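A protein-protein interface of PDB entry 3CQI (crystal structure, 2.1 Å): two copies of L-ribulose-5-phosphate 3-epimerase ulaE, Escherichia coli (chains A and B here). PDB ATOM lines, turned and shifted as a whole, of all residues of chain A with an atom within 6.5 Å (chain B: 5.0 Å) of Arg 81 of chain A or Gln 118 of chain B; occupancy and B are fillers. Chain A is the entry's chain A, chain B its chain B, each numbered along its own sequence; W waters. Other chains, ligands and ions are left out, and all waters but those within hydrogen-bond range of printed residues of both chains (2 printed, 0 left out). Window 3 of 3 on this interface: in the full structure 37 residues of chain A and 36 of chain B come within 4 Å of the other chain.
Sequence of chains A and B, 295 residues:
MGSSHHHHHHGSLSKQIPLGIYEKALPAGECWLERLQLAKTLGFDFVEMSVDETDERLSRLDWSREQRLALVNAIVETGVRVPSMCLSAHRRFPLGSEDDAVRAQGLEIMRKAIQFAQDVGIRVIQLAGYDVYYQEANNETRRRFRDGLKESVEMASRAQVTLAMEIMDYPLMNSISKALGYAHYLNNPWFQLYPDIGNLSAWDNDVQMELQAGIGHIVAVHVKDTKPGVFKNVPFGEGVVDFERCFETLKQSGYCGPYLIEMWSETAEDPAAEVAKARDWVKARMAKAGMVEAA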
ATOM      1  N   LEU A  36     -32.745   3.212  -7.101  1.00  0.00           N
ATOM      2  CA  LEU A  36     -31.502   3.396  -6.324  1.00  0.00           C
ATOM      3  C   LEU A  36     -30.602   2.160  -6.345  1.00  0.00           C
ATOM      4  O   LEU A  36     -29.379   2.283  -6.427  1.00  0.00           O
ATOM      5  CB  LEU A  36     -31.815   3.812  -4.881  1.00  0.00           C
ATOM      6  CG  LEU A  36     -32.517   5.164  -4.726  1.00  0.00           C
ATOM      7  CD1 LEU A  36     -32.882   5.442  -3.259  1.00  0.00           C
ATOM      8  CD2 LEU A  36     -31.660   6.300  -5.303  1.00  0.00           C
ATOM      9  N   ASP A  45     -23.036   6.943  -6.957  1.00  0.00           N
ATOM     10  CA  ASP A  45     -23.072   7.238  -5.539  1.00  0.00           C
ATOM     11  C   ASP A  45     -24.381   7.921  -5.195  1.00  0.00           C
ATOM     12  O   ASP A  45     -24.786   7.936  -4.029  1.00  0.00           O
ATOM     13  CB  ASP A  45     -21.903   8.156  -5.182  1.00  0.00           C
ATOM     14  CG  ASP A  45     -20.569   7.573  -5.599  1.00  0.00           C
ATOM     15  OD1 ASP A  45     -20.247   6.474  -5.100  1.00  0.00           O
ATOM     16  OD2 ASP A  45     -19.853   8.197  -6.418  1.00  0.00           O
ATOM     17  N   PHE A  46     -25.018   8.522  -6.201  1.00  0.00           N
ATOM     18  CA  PHE A  46     -26.292   9.217  -6.002  1.00  0.00           C
ATOM     19  C   PHE A  46     -27.141   9.313  -7.261  1.00  0.00           C
ATOM     20  O   PHE A  46     -26.676   9.023  -8.361  1.00  0.00           O
ATOM     21  CB  PHE A  46     -26.083  10.610  -5.359  1.00  0.00           C
ATOM     22  CG  PHE A  46     -25.399  11.635  -6.249  1.00  0.00           C
ATOM     23  CD1 PHE A  46     -26.144  12.598  -6.918  1.00  0.00           C
ATOM     24  CD2 PHE A  46     -24.015  11.672  -6.360  1.00  0.00           C
ATOM     25  CE1 PHE A  46     -25.529  13.571  -7.687  1.00  0.00           C
ATOM     26  CE2 PHE A  46     -23.381  12.635  -7.144  1.00  0.00           C
ATOM     27  CZ  PHE A  46     -24.143  13.584  -7.813  1.00  0.00           C
ATOM     28  N   VAL A  47     -28.405   9.691  -7.073  1.00  0.00           N
ATOM     29  CA  VAL A  47     -29.314   9.978  -8.158  1.00  0.00           C
ATOM     30  C   VAL A  47     -29.878  11.353  -7.875  1.00  0.00           C
ATOM     31  O   VAL A  47     -30.161  11.691  -6.721  1.00  0.00           O
ATOM     32  CB  VAL A  47     -30.498   8.946  -8.238  1.00  0.00           C
ATOM     33  CG1 VAL A  47     -31.521   9.356  -9.302  1.00  0.00           C
ATOM     34  CG2 VAL A  47     -29.982   7.535  -8.526  1.00  0.00           C
ATOM     35  N   GLU A  48     -30.031  12.154  -8.921  1.00  0.00           N
ATOM     36  CA  GLU A  48     -30.686  13.425  -8.778  1.00  0.00           C
ATOM     37  C   GLU A  48     -32.145  13.298  -9.221  1.00  0.00           C
ATOM     38  O   GLU A  48     -32.424  12.900 -10.333  1.00  0.00           O
ATOM     39  CB  GLU A  48     -29.934  14.506  -9.553  1.00  0.00           C
ATOM     40  CG  GLU A  48     -30.660  15.839  -9.654  1.00  0.00           C
ATOM     41  CD  GLU A  48     -29.756  16.913 -10.208  1.00  0.00           C
ATOM     42  OE1 GLU A  48     -29.862  17.206 -11.420  1.00  0.00           O
ATOM     43  OE2 GLU A  48     -28.904  17.416  -9.443  1.00  0.00           O
ATOM     44  N   ILE A  75     -33.072   5.081   0.467  1.00  0.00           N
ATOM     45  CA  ILE A  75     -31.761   5.750   0.463  1.00  0.00           C
ATOM     46  C   ILE A  75     -30.843   5.161   1.541  1.00  0.00           C
ATOM     47  O   ILE A  75     -29.696   4.802   1.277  1.00  0.00           O
ATOM     48  CB  ILE A  75     -31.919   7.275   0.682  1.00  0.00           C
ATOM     49  CG1 ILE A  75     -32.555   7.921  -0.552  1.00  0.00           C
ATOM     50  CG2 ILE A  75     -30.574   7.920   1.069  1.00  0.00           C
ATOM     51  CD1 ILE A  75     -33.172   9.288  -0.292  1.00  0.00           C
ATOM     52  N   VAL A  76     -31.368   5.045   2.753  1.00  0.00           N
ATOM     53  CA  VAL A  76     -30.587   4.532   3.884  1.00  0.00           C
ATOM     54  C   VAL A  76     -30.205   3.058   3.655  1.00  0.00           C
ATOM     55  O   VAL A  76     -29.104   2.639   3.986  1.00  0.00           O
ATOM     56  CB  VAL A  76     -31.332   4.780   5.231  1.00  0.00           C
ATOM     57  CG1 VAL A  76     -30.835   3.851   6.337  1.00  0.00           C
ATOM     58  CG2 VAL A  76     -31.179   6.242   5.659  1.00  0.00           C
ATOM     59  N   THR A  78     -29.976   1.310   0.571  1.00  0.00           N
ATOM     60  CA  THR A  78     -29.083   1.106  -0.577  1.00  0.00           C
ATOM     61  C   THR A  78     -27.747   1.812  -0.422  1.00  0.00           C
ATOM     62  O   THR A  78     -26.760   1.401  -1.042  1.00  0.00           O
ATOM     63  CB  THR A  78     -29.709   1.584  -1.912  1.00  0.00           C
ATOM     64  OG1 THR A  78     -30.054   2.978  -1.819  1.00  0.00           O
ATOM     65  CG2 THR A  78     -30.944   0.770  -2.249  1.00  0.00           C
ATOM     66  N   GLY A  79     -27.721   2.870   0.393  1.00  0.00           N
ATOM     67  CA  GLY A  79     -26.562   3.758   0.480  1.00  0.00           C
ATOM     68  C   GLY A  79     -26.420   4.757  -0.667  1.00  0.00           C
ATOM     69  O   GLY A  79     -25.436   5.506  -0.727  1.00  0.00           O
ATOM     70  N   VAL A  80     -27.388   4.772  -1.584  1.00  0.00           N
ATOM     71  CA  VAL A  80     -27.361   5.680  -2.734  1.00  0.00           C
ATOM     72  C   VAL A  80     -28.186   6.909  -2.397  1.00  0.00           C
ATOM     73  O   VAL A  80     -29.401   6.798  -2.200  1.00  0.00           O
ATOM     74  CB  VAL A  80     -27.914   4.998  -4.015  1.00  0.00           C
ATOM     75  CG1 VAL A  80     -27.869   5.956  -5.228  1.00  0.00           C
ATOM     76  CG2 VAL A  80     -27.138   3.719  -4.308  1.00  0.00           C
ATOM     77  N   ARG A  81     -27.534   8.073  -2.328  1.00  0.00           N
ATOM     78  CA  ARG A  81     -28.198   9.319  -1.912  1.00  0.00           C
ATOM     79  C   ARG A  81     -29.080   9.937  -2.998  1.00  0.00           C
ATOM     80  O   ARG A  81     -28.914   9.656  -4.187  1.00  0.00           O
ATOM     81  CB  ARG A  81     -27.177  10.373  -1.430  1.00  0.00           C
ATOM     82  CG  ARG A  81     -26.211   9.921  -0.328  1.00  0.00           C
ATOM     83  CD  ARG A  81     -26.918   9.730   0.991  1.00  0.00           C
ATOM     84  NE  ARG A  81     -26.013   9.276   2.044  1.00  0.00           N
ATOM     85  CZ  ARG A  81     -26.411   8.913   3.267  1.00  0.00           C
ATOM     86  NH1 ARG A  81     -27.708   8.950   3.599  1.00  0.00           N
ATOM     87  NH2 ARG A  81     -25.506   8.511   4.160  1.00  0.00           N
ATOM     88  N   VAL A  82     -30.035  10.764  -2.567  1.00  0.00           N
ATOM     89  CA  VAL A  82     -30.743  11.687  -3.453  1.00  0.00           C
ATOM     90  C   VAL A  82     -30.457  13.070  -2.862  1.00  0.00           C
ATOM     91  O   VAL A  82     -31.281  13.622  -2.124  1.00  0.00           O
ATOM     92  CB  VAL A  82     -32.273  11.392  -3.562  1.00  0.00           C
ATOM     93  CG1 VAL A  82     -32.954  12.332  -4.569  1.00  0.00           C
ATOM     94  CG2 VAL A  82     -32.516   9.929  -3.973  1.00  0.00           C
ATOM     95  N   PRO A  83     -29.247  13.607  -3.133  1.00  0.00           N
ATOM     96  CA  PRO A  83     -28.829  14.883  -2.518  1.00  0.00           C
ATOM     97  C   PRO A  83     -29.364  16.109  -3.234  1.00  0.00           C
ATOM     98  O   PRO A  83     -29.284  17.225  -2.711  1.00  0.00           O
ATOM     99  CB  PRO A  83     -27.299  14.848  -2.656  1.00  0.00           C
ATOM    100  CG  PRO A  83     -27.050  14.080  -3.908  1.00  0.00           C
ATOM    101  CD  PRO A  83     -28.189  13.043  -3.999  1.00  0.00           C
ATOM    102  N   SER A  84     -29.851  15.924  -4.453  1.00  0.00           N
ATOM    103  CA  SER A  84     -30.320  17.059  -5.211  1.00  0.00           C
ATOM    104  C   SER A  84     -31.608  16.785  -5.966  1.00  0.00           C
ATOM    105  O   SER A  84     -31.979  15.636  -6.211  1.00  0.00           O
ATOM    106  CB  SER A  84     -29.219  17.619  -6.129  1.00  0.00           C
ATOM    107  OG  SER A  84     -28.618  16.602  -6.901  1.00  0.00           O
ATOM    108  N   VAL A 120     -37.227  14.732   3.081  1.00  0.00           N
ATOM    109  CA  VAL A 120     -36.465  13.563   2.607  1.00  0.00           C
ATOM    110  C   VAL A 120     -34.941  13.722   2.626  1.00  0.00           C
ATOM    111  O   VAL A 120     -34.215  12.792   2.249  1.00  0.00           O
ATOM    112  CB  VAL A 120     -36.922  13.068   1.213  1.00  0.00           C
ATOM    113  CG1 VAL A 120     -38.423  12.753   1.217  1.00  0.00           C
ATOM    114  CG2 VAL A 120     -36.570  14.079   0.138  1.00  0.00           C
ATOM    115  N   GLY A 121     -34.465  14.878   3.087  1.00  0.00           N
ATOM    116  CA  GLY A 121     -33.029  15.105   3.305  1.00  0.00           C
ATOM    117  C   GLY A 121     -32.267  15.510   2.053  1.00  0.00           C
ATOM    118  O   GLY A 121     -31.054  15.257   1.945  1.00  0.00           O
ATOM    119  N   ARG A 123     -30.235  17.821  -0.198  1.00  0.00           N
ATOM    120  CA  ARG A 123     -29.259  18.850   0.141  1.00  0.00           C
ATOM    121  C   ARG A 123     -29.429  20.124  -0.667  1.00  0.00           C
ATOM    122  O   ARG A 123     -29.290  21.228  -0.130  1.00  0.00           O
ATOM    123  CB  ARG A 123     -27.861  18.290  -0.104  1.00  0.00           C
ATOM    124  CG  ARG A 123     -27.543  17.180   0.852  1.00  0.00           C
ATOM    125  CD  ARG A 123     -27.175  17.884   2.143  1.00  0.00           C
ATOM    126  NE  ARG A 123     -27.840  17.287   3.243  1.00  0.00           N
ATOM    127  CZ  ARG A 123     -27.886  17.772   4.468  1.00  0.00           C
ATOM    128  NH1 ARG A 123     -27.319  18.928   4.809  1.00  0.00           N
ATOM    129  NH2 ARG A 123     -28.537  17.057   5.343  1.00  0.00           N
ATOM    130  N   ILE B 114     -20.971  14.147   9.623  1.00  0.00           N
ATOM    131  CA  ILE B 114     -21.430  14.508   8.278  1.00  0.00           C
ATOM    132  C   ILE B 114     -22.343  13.431   7.724  1.00  0.00           C
ATOM    133  O   ILE B 114     -23.414  13.729   7.217  1.00  0.00           O
ATOM    134  CB  ILE B 114     -20.247  14.784   7.323  1.00  0.00           C
ATOM    135  CG1 ILE B 114     -19.585  16.117   7.721  1.00  0.00           C
ATOM    136  CG2 ILE B 114     -20.737  14.863   5.851  1.00  0.00           C
ATOM    137  CD1 ILE B 114     -18.235  16.386   7.088  1.00  0.00           C
ATOM    138  N   GLN B 115     -21.901  12.184   7.827  1.00  0.00           N
ATOM    139  CA  GLN B 115     -22.710  11.023   7.450  1.00  0.00           C
ATOM    140  C   GLN B 115     -24.043  10.955   8.222  1.00  0.00           C
ATOM    141  O   GLN B 115     -25.102  10.713   7.621  1.00  0.00           O
ATOM    142  CB  GLN B 115     -21.878   9.757   7.650  1.00  0.00           C
ATOM    143  CG  GLN B 115     -22.587   8.460   7.291  1.00  0.00           C
ATOM    144  CD  GLN B 115     -21.693   7.272   7.543  1.00  0.00           C
ATOM    145  OE1 GLN B 115     -21.421   6.909   8.695  1.00  0.00           O
ATOM    146  NE2 GLN B 115     -21.195   6.676   6.465  1.00  0.00           N
ATOM    147  N   PHE B 116     -23.997  11.153   9.539  1.00  0.00           N
ATOM    148  CA  PHE B 116     -25.205  11.257  10.372  1.00  0.00           C
ATOM    149  C   PHE B 116     -26.157  12.374   9.893  1.00  0.00           C
ATOM    150  O   PHE B 116     -27.365  12.153   9.771  1.00  0.00           O
ATOM    151  CB  PHE B 116     -24.796  11.524  11.819  1.00  0.00           C
ATOM    152  CG  PHE B 116     -25.919  11.419  12.818  1.00  0.00           C
ATOM    153  CD1 PHE B 116     -26.133  10.234  13.525  1.00  0.00           C
ATOM    154  CD2 PHE B 116     -26.713  12.523  13.111  1.00  0.00           C
ATOM    155  CE1 PHE B 116     -27.157  10.157  14.490  1.00  0.00           C
ATOM    156  CE2 PHE B 116     -27.732  12.446  14.057  1.00  0.00           C
ATOM    157  CZ  PHE B 116     -27.952  11.279  14.757  1.00  0.00           C
ATOM    158  N   ALA B 117     -25.627  13.567   9.630  1.00  0.00           N
ATOM    159  CA  ALA B 117     -26.454  14.658   9.053  1.00  0.00           C
ATOM    160  C   ALA B 117     -27.100  14.292   7.710  1.00  0.00           C
ATOM    161  O   ALA B 117     -28.253  14.665   7.450  1.00  0.00           O
ATOM    162  CB  ALA B 117     -25.637  15.971   8.937  1.00  0.00           C
ATOM    163  N   GLN B 118     -26.373  13.560   6.861  1.00  0.00           N
ATOM    164  CA  GLN B 118     -26.926  13.053   5.589  1.00  0.00           C
ATOM    165  C   GLN B 118     -28.102  12.090   5.831  1.00  0.00           C
ATOM    166  O   GLN B 118     -29.146  12.183   5.173  1.00  0.00           O
ATOM    167  CB  GLN B 118     -25.864  12.299   4.772  1.00  0.00           C
ATOM    168  CG  GLN B 118     -24.764  13.141   4.096  1.00  0.00           C
ATOM    169  CD  GLN B 118     -23.726  12.261   3.387  1.00  0.00           C
ATOM    170  OE1 GLN B 118     -22.928  11.579   4.039  1.00  0.00           O
ATOM    171  NE2 GLN B 118     -23.726  12.283   2.048  1.00  0.00           N
ATOM    172  N   ASP B 119     -27.904  11.155   6.755  1.00  0.00           N
ATOM    173  CA  ASP B 119     -28.876  10.103   7.038  1.00  0.00           C
ATOM    174  C   ASP B 119     -30.178  10.692   7.590  1.00  0.00           C
ATOM    175  O   ASP B 119     -31.275  10.314   7.181  1.00  0.00           O
ATOM    176  CB  ASP B 119     -28.303   9.101   8.047  1.00  0.00           C
ATOM    177  CG  ASP B 119     -27.196   8.213   7.465  1.00  0.00           C
ATOM    178  OD1 ASP B 119     -27.004   8.158   6.227  1.00  0.00           O
ATOM    179  OD2 ASP B 119     -26.504   7.552   8.269  1.00  0.00           O
ATOM    180  N   VAL B 120     -30.031  11.666   8.477  1.00  0.00           N
ATOM    181  CA  VAL B 120     -31.131  12.182   9.283  1.00  0.00           C
ATOM    182  C   VAL B 120     -31.665  13.531   8.798  1.00  0.00           C
ATOM    183  O   VAL B 120     -32.563  14.111   9.416  1.00  0.00           O
ATOM    184  CB  VAL B 120     -30.668  12.263  10.751  1.00  0.00           C
ATOM    185  CG1 VAL B 120     -31.636  13.078  11.590  1.00  0.00           C
ATOM    186  CG2 VAL B 120     -30.517  10.847  11.312  1.00  0.00           C
ATOM    187  N   GLY B 121     -31.119  14.031   7.694  1.00  0.00           N
ATOM    188  CA  GLY B 121     -31.561  15.302   7.118  1.00  0.00           C
ATOM    189  C   GLY B 121     -31.227  16.556   7.918  1.00  0.00           C
ATOM    190  O   GLY B 121     -31.906  17.590   7.782  1.00  0.00           O
ATOM    191  N   ALA B 159     -20.528  15.632   0.469  1.00  0.00           N
ATOM    192  CA  ALA B 159     -21.792  15.271   1.075  1.00  0.00           C
ATOM    193  C   ALA B 159     -22.846  16.365   0.890  1.00  0.00           C
ATOM    194  O   ALA B 159     -24.060  16.105   1.013  1.00  0.00           O
ATOM    195  CB  ALA B 159     -21.587  14.975   2.552  1.00  0.00           C
ATOM    196  N   VAL B 161     -23.187  19.131   2.839  1.00  0.00           N
ATOM    197  CA  VAL B 161     -23.707  19.404   4.173  1.00  0.00           C
ATOM    198  C   VAL B 161     -23.001  20.677   4.632  1.00  0.00           C
ATOM    199  O   VAL B 161     -21.788  20.790   4.477  1.00  0.00           O
ATOM    200  CB  VAL B 161     -23.386  18.239   5.147  1.00  0.00           C
ATOM    201  CG1 VAL B 161     -23.635  18.648   6.645  1.00  0.00           C
ATOM    202  CG2 VAL B 161     -24.181  16.990   4.770  1.00  0.00           C
HETATM  203  O   HOH W   1     -29.609  14.577   4.000  1.00  0.00           O
HETATM  204  O   HOH W   2     -29.756  10.825   3.127  1.00  0.00           O
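The side-chain carboxylate (OD1) of Asp 119 of chain B lies within salt-bridge range of the guanidinium group (NH2) of Arg 81 of chain A, 2.6 Å away.
NH2 of Arg 123 of chain A lies within hydrogen-bond range of O of Ala 117 of chain B (3.2 Å).
2 positions are printed for both chains.
Printed residues of chain B within 4 Å of Arg 81 of chain A: Gln 118 and Asp 119.
Of the printed residues of chain B, Arg 123 of chain A touches Ala 117, Gly 121, Ala 159 and Val 161.
Ile 114 of chain B touches none of the printed residues of chain A.
Gln 118 of chain B touches just one residue of chain A: Arg 81 (3.7 Å).
Printed residues of chain A within 4 Å of Asp 119 of chain B: Arg 81 (2.6 Å).
Of the printed residues of chain A, Gly 121 of chain B touches Arg 123.
Of the printed residues of chain A, Ala 159 of chain B touches Arg 123 (3.6 Å).
Of the printed residues of chain A, Val 161 of chain B touches Arg 123 (3.7 Å).
The nearest printed residue of chain A that does not touch Gly 121 of chain B is Gly 121 of chain A (4.1 Å).
The backbone carbonyl oxygen of Asp 45 of chain A lies within hydrogen-bond range of the backbone NH of Arg 81 of chain A (3.2 Å).
O of Pro 83 of chain A sits at hydrogen-bond distance from N of Arg 123 of chain A (2.8 Å).
N of Val 47 of chain A sits at hydrogen-bond distance from O of Arg 81 of chain A.
Gln 118 of chain B touches Arg 81 of chain A.
NH2 of Arg 123 of chain A touches C of Gly 121 of chain B (3.8 Å).
Arg 123 of chain A touches Ala 159 of chain B.
Val 161 of chain B touches Arg 123 of chain A.
Water W2 lies within hydrogen-bond range of O of Gln 118 of chain B (2.5 Å) and NH1 of Arg 81 of chain A (2.8 Å).
Water W1 lies within hydrogen-bond range of O of Gly 121 of chain A (2.6 Å), O of Gln 118 of chain B (2.7 Å) and NH2 of Arg 123 of chain A (3.0 Å).
Hydrophobic or aromatic side chains of chain B that line the printed part of chain A: Val 161.
Printed residues of chain A that touch a printed residue of chain B: Arg 81 and Arg 123.
Among the printed residues, Asp or Glu carboxylates within 4 Å of a Lys or Arg side-chain nitrogen of the other chain: Arg 81 of chain A with Asp 119 of chain B.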
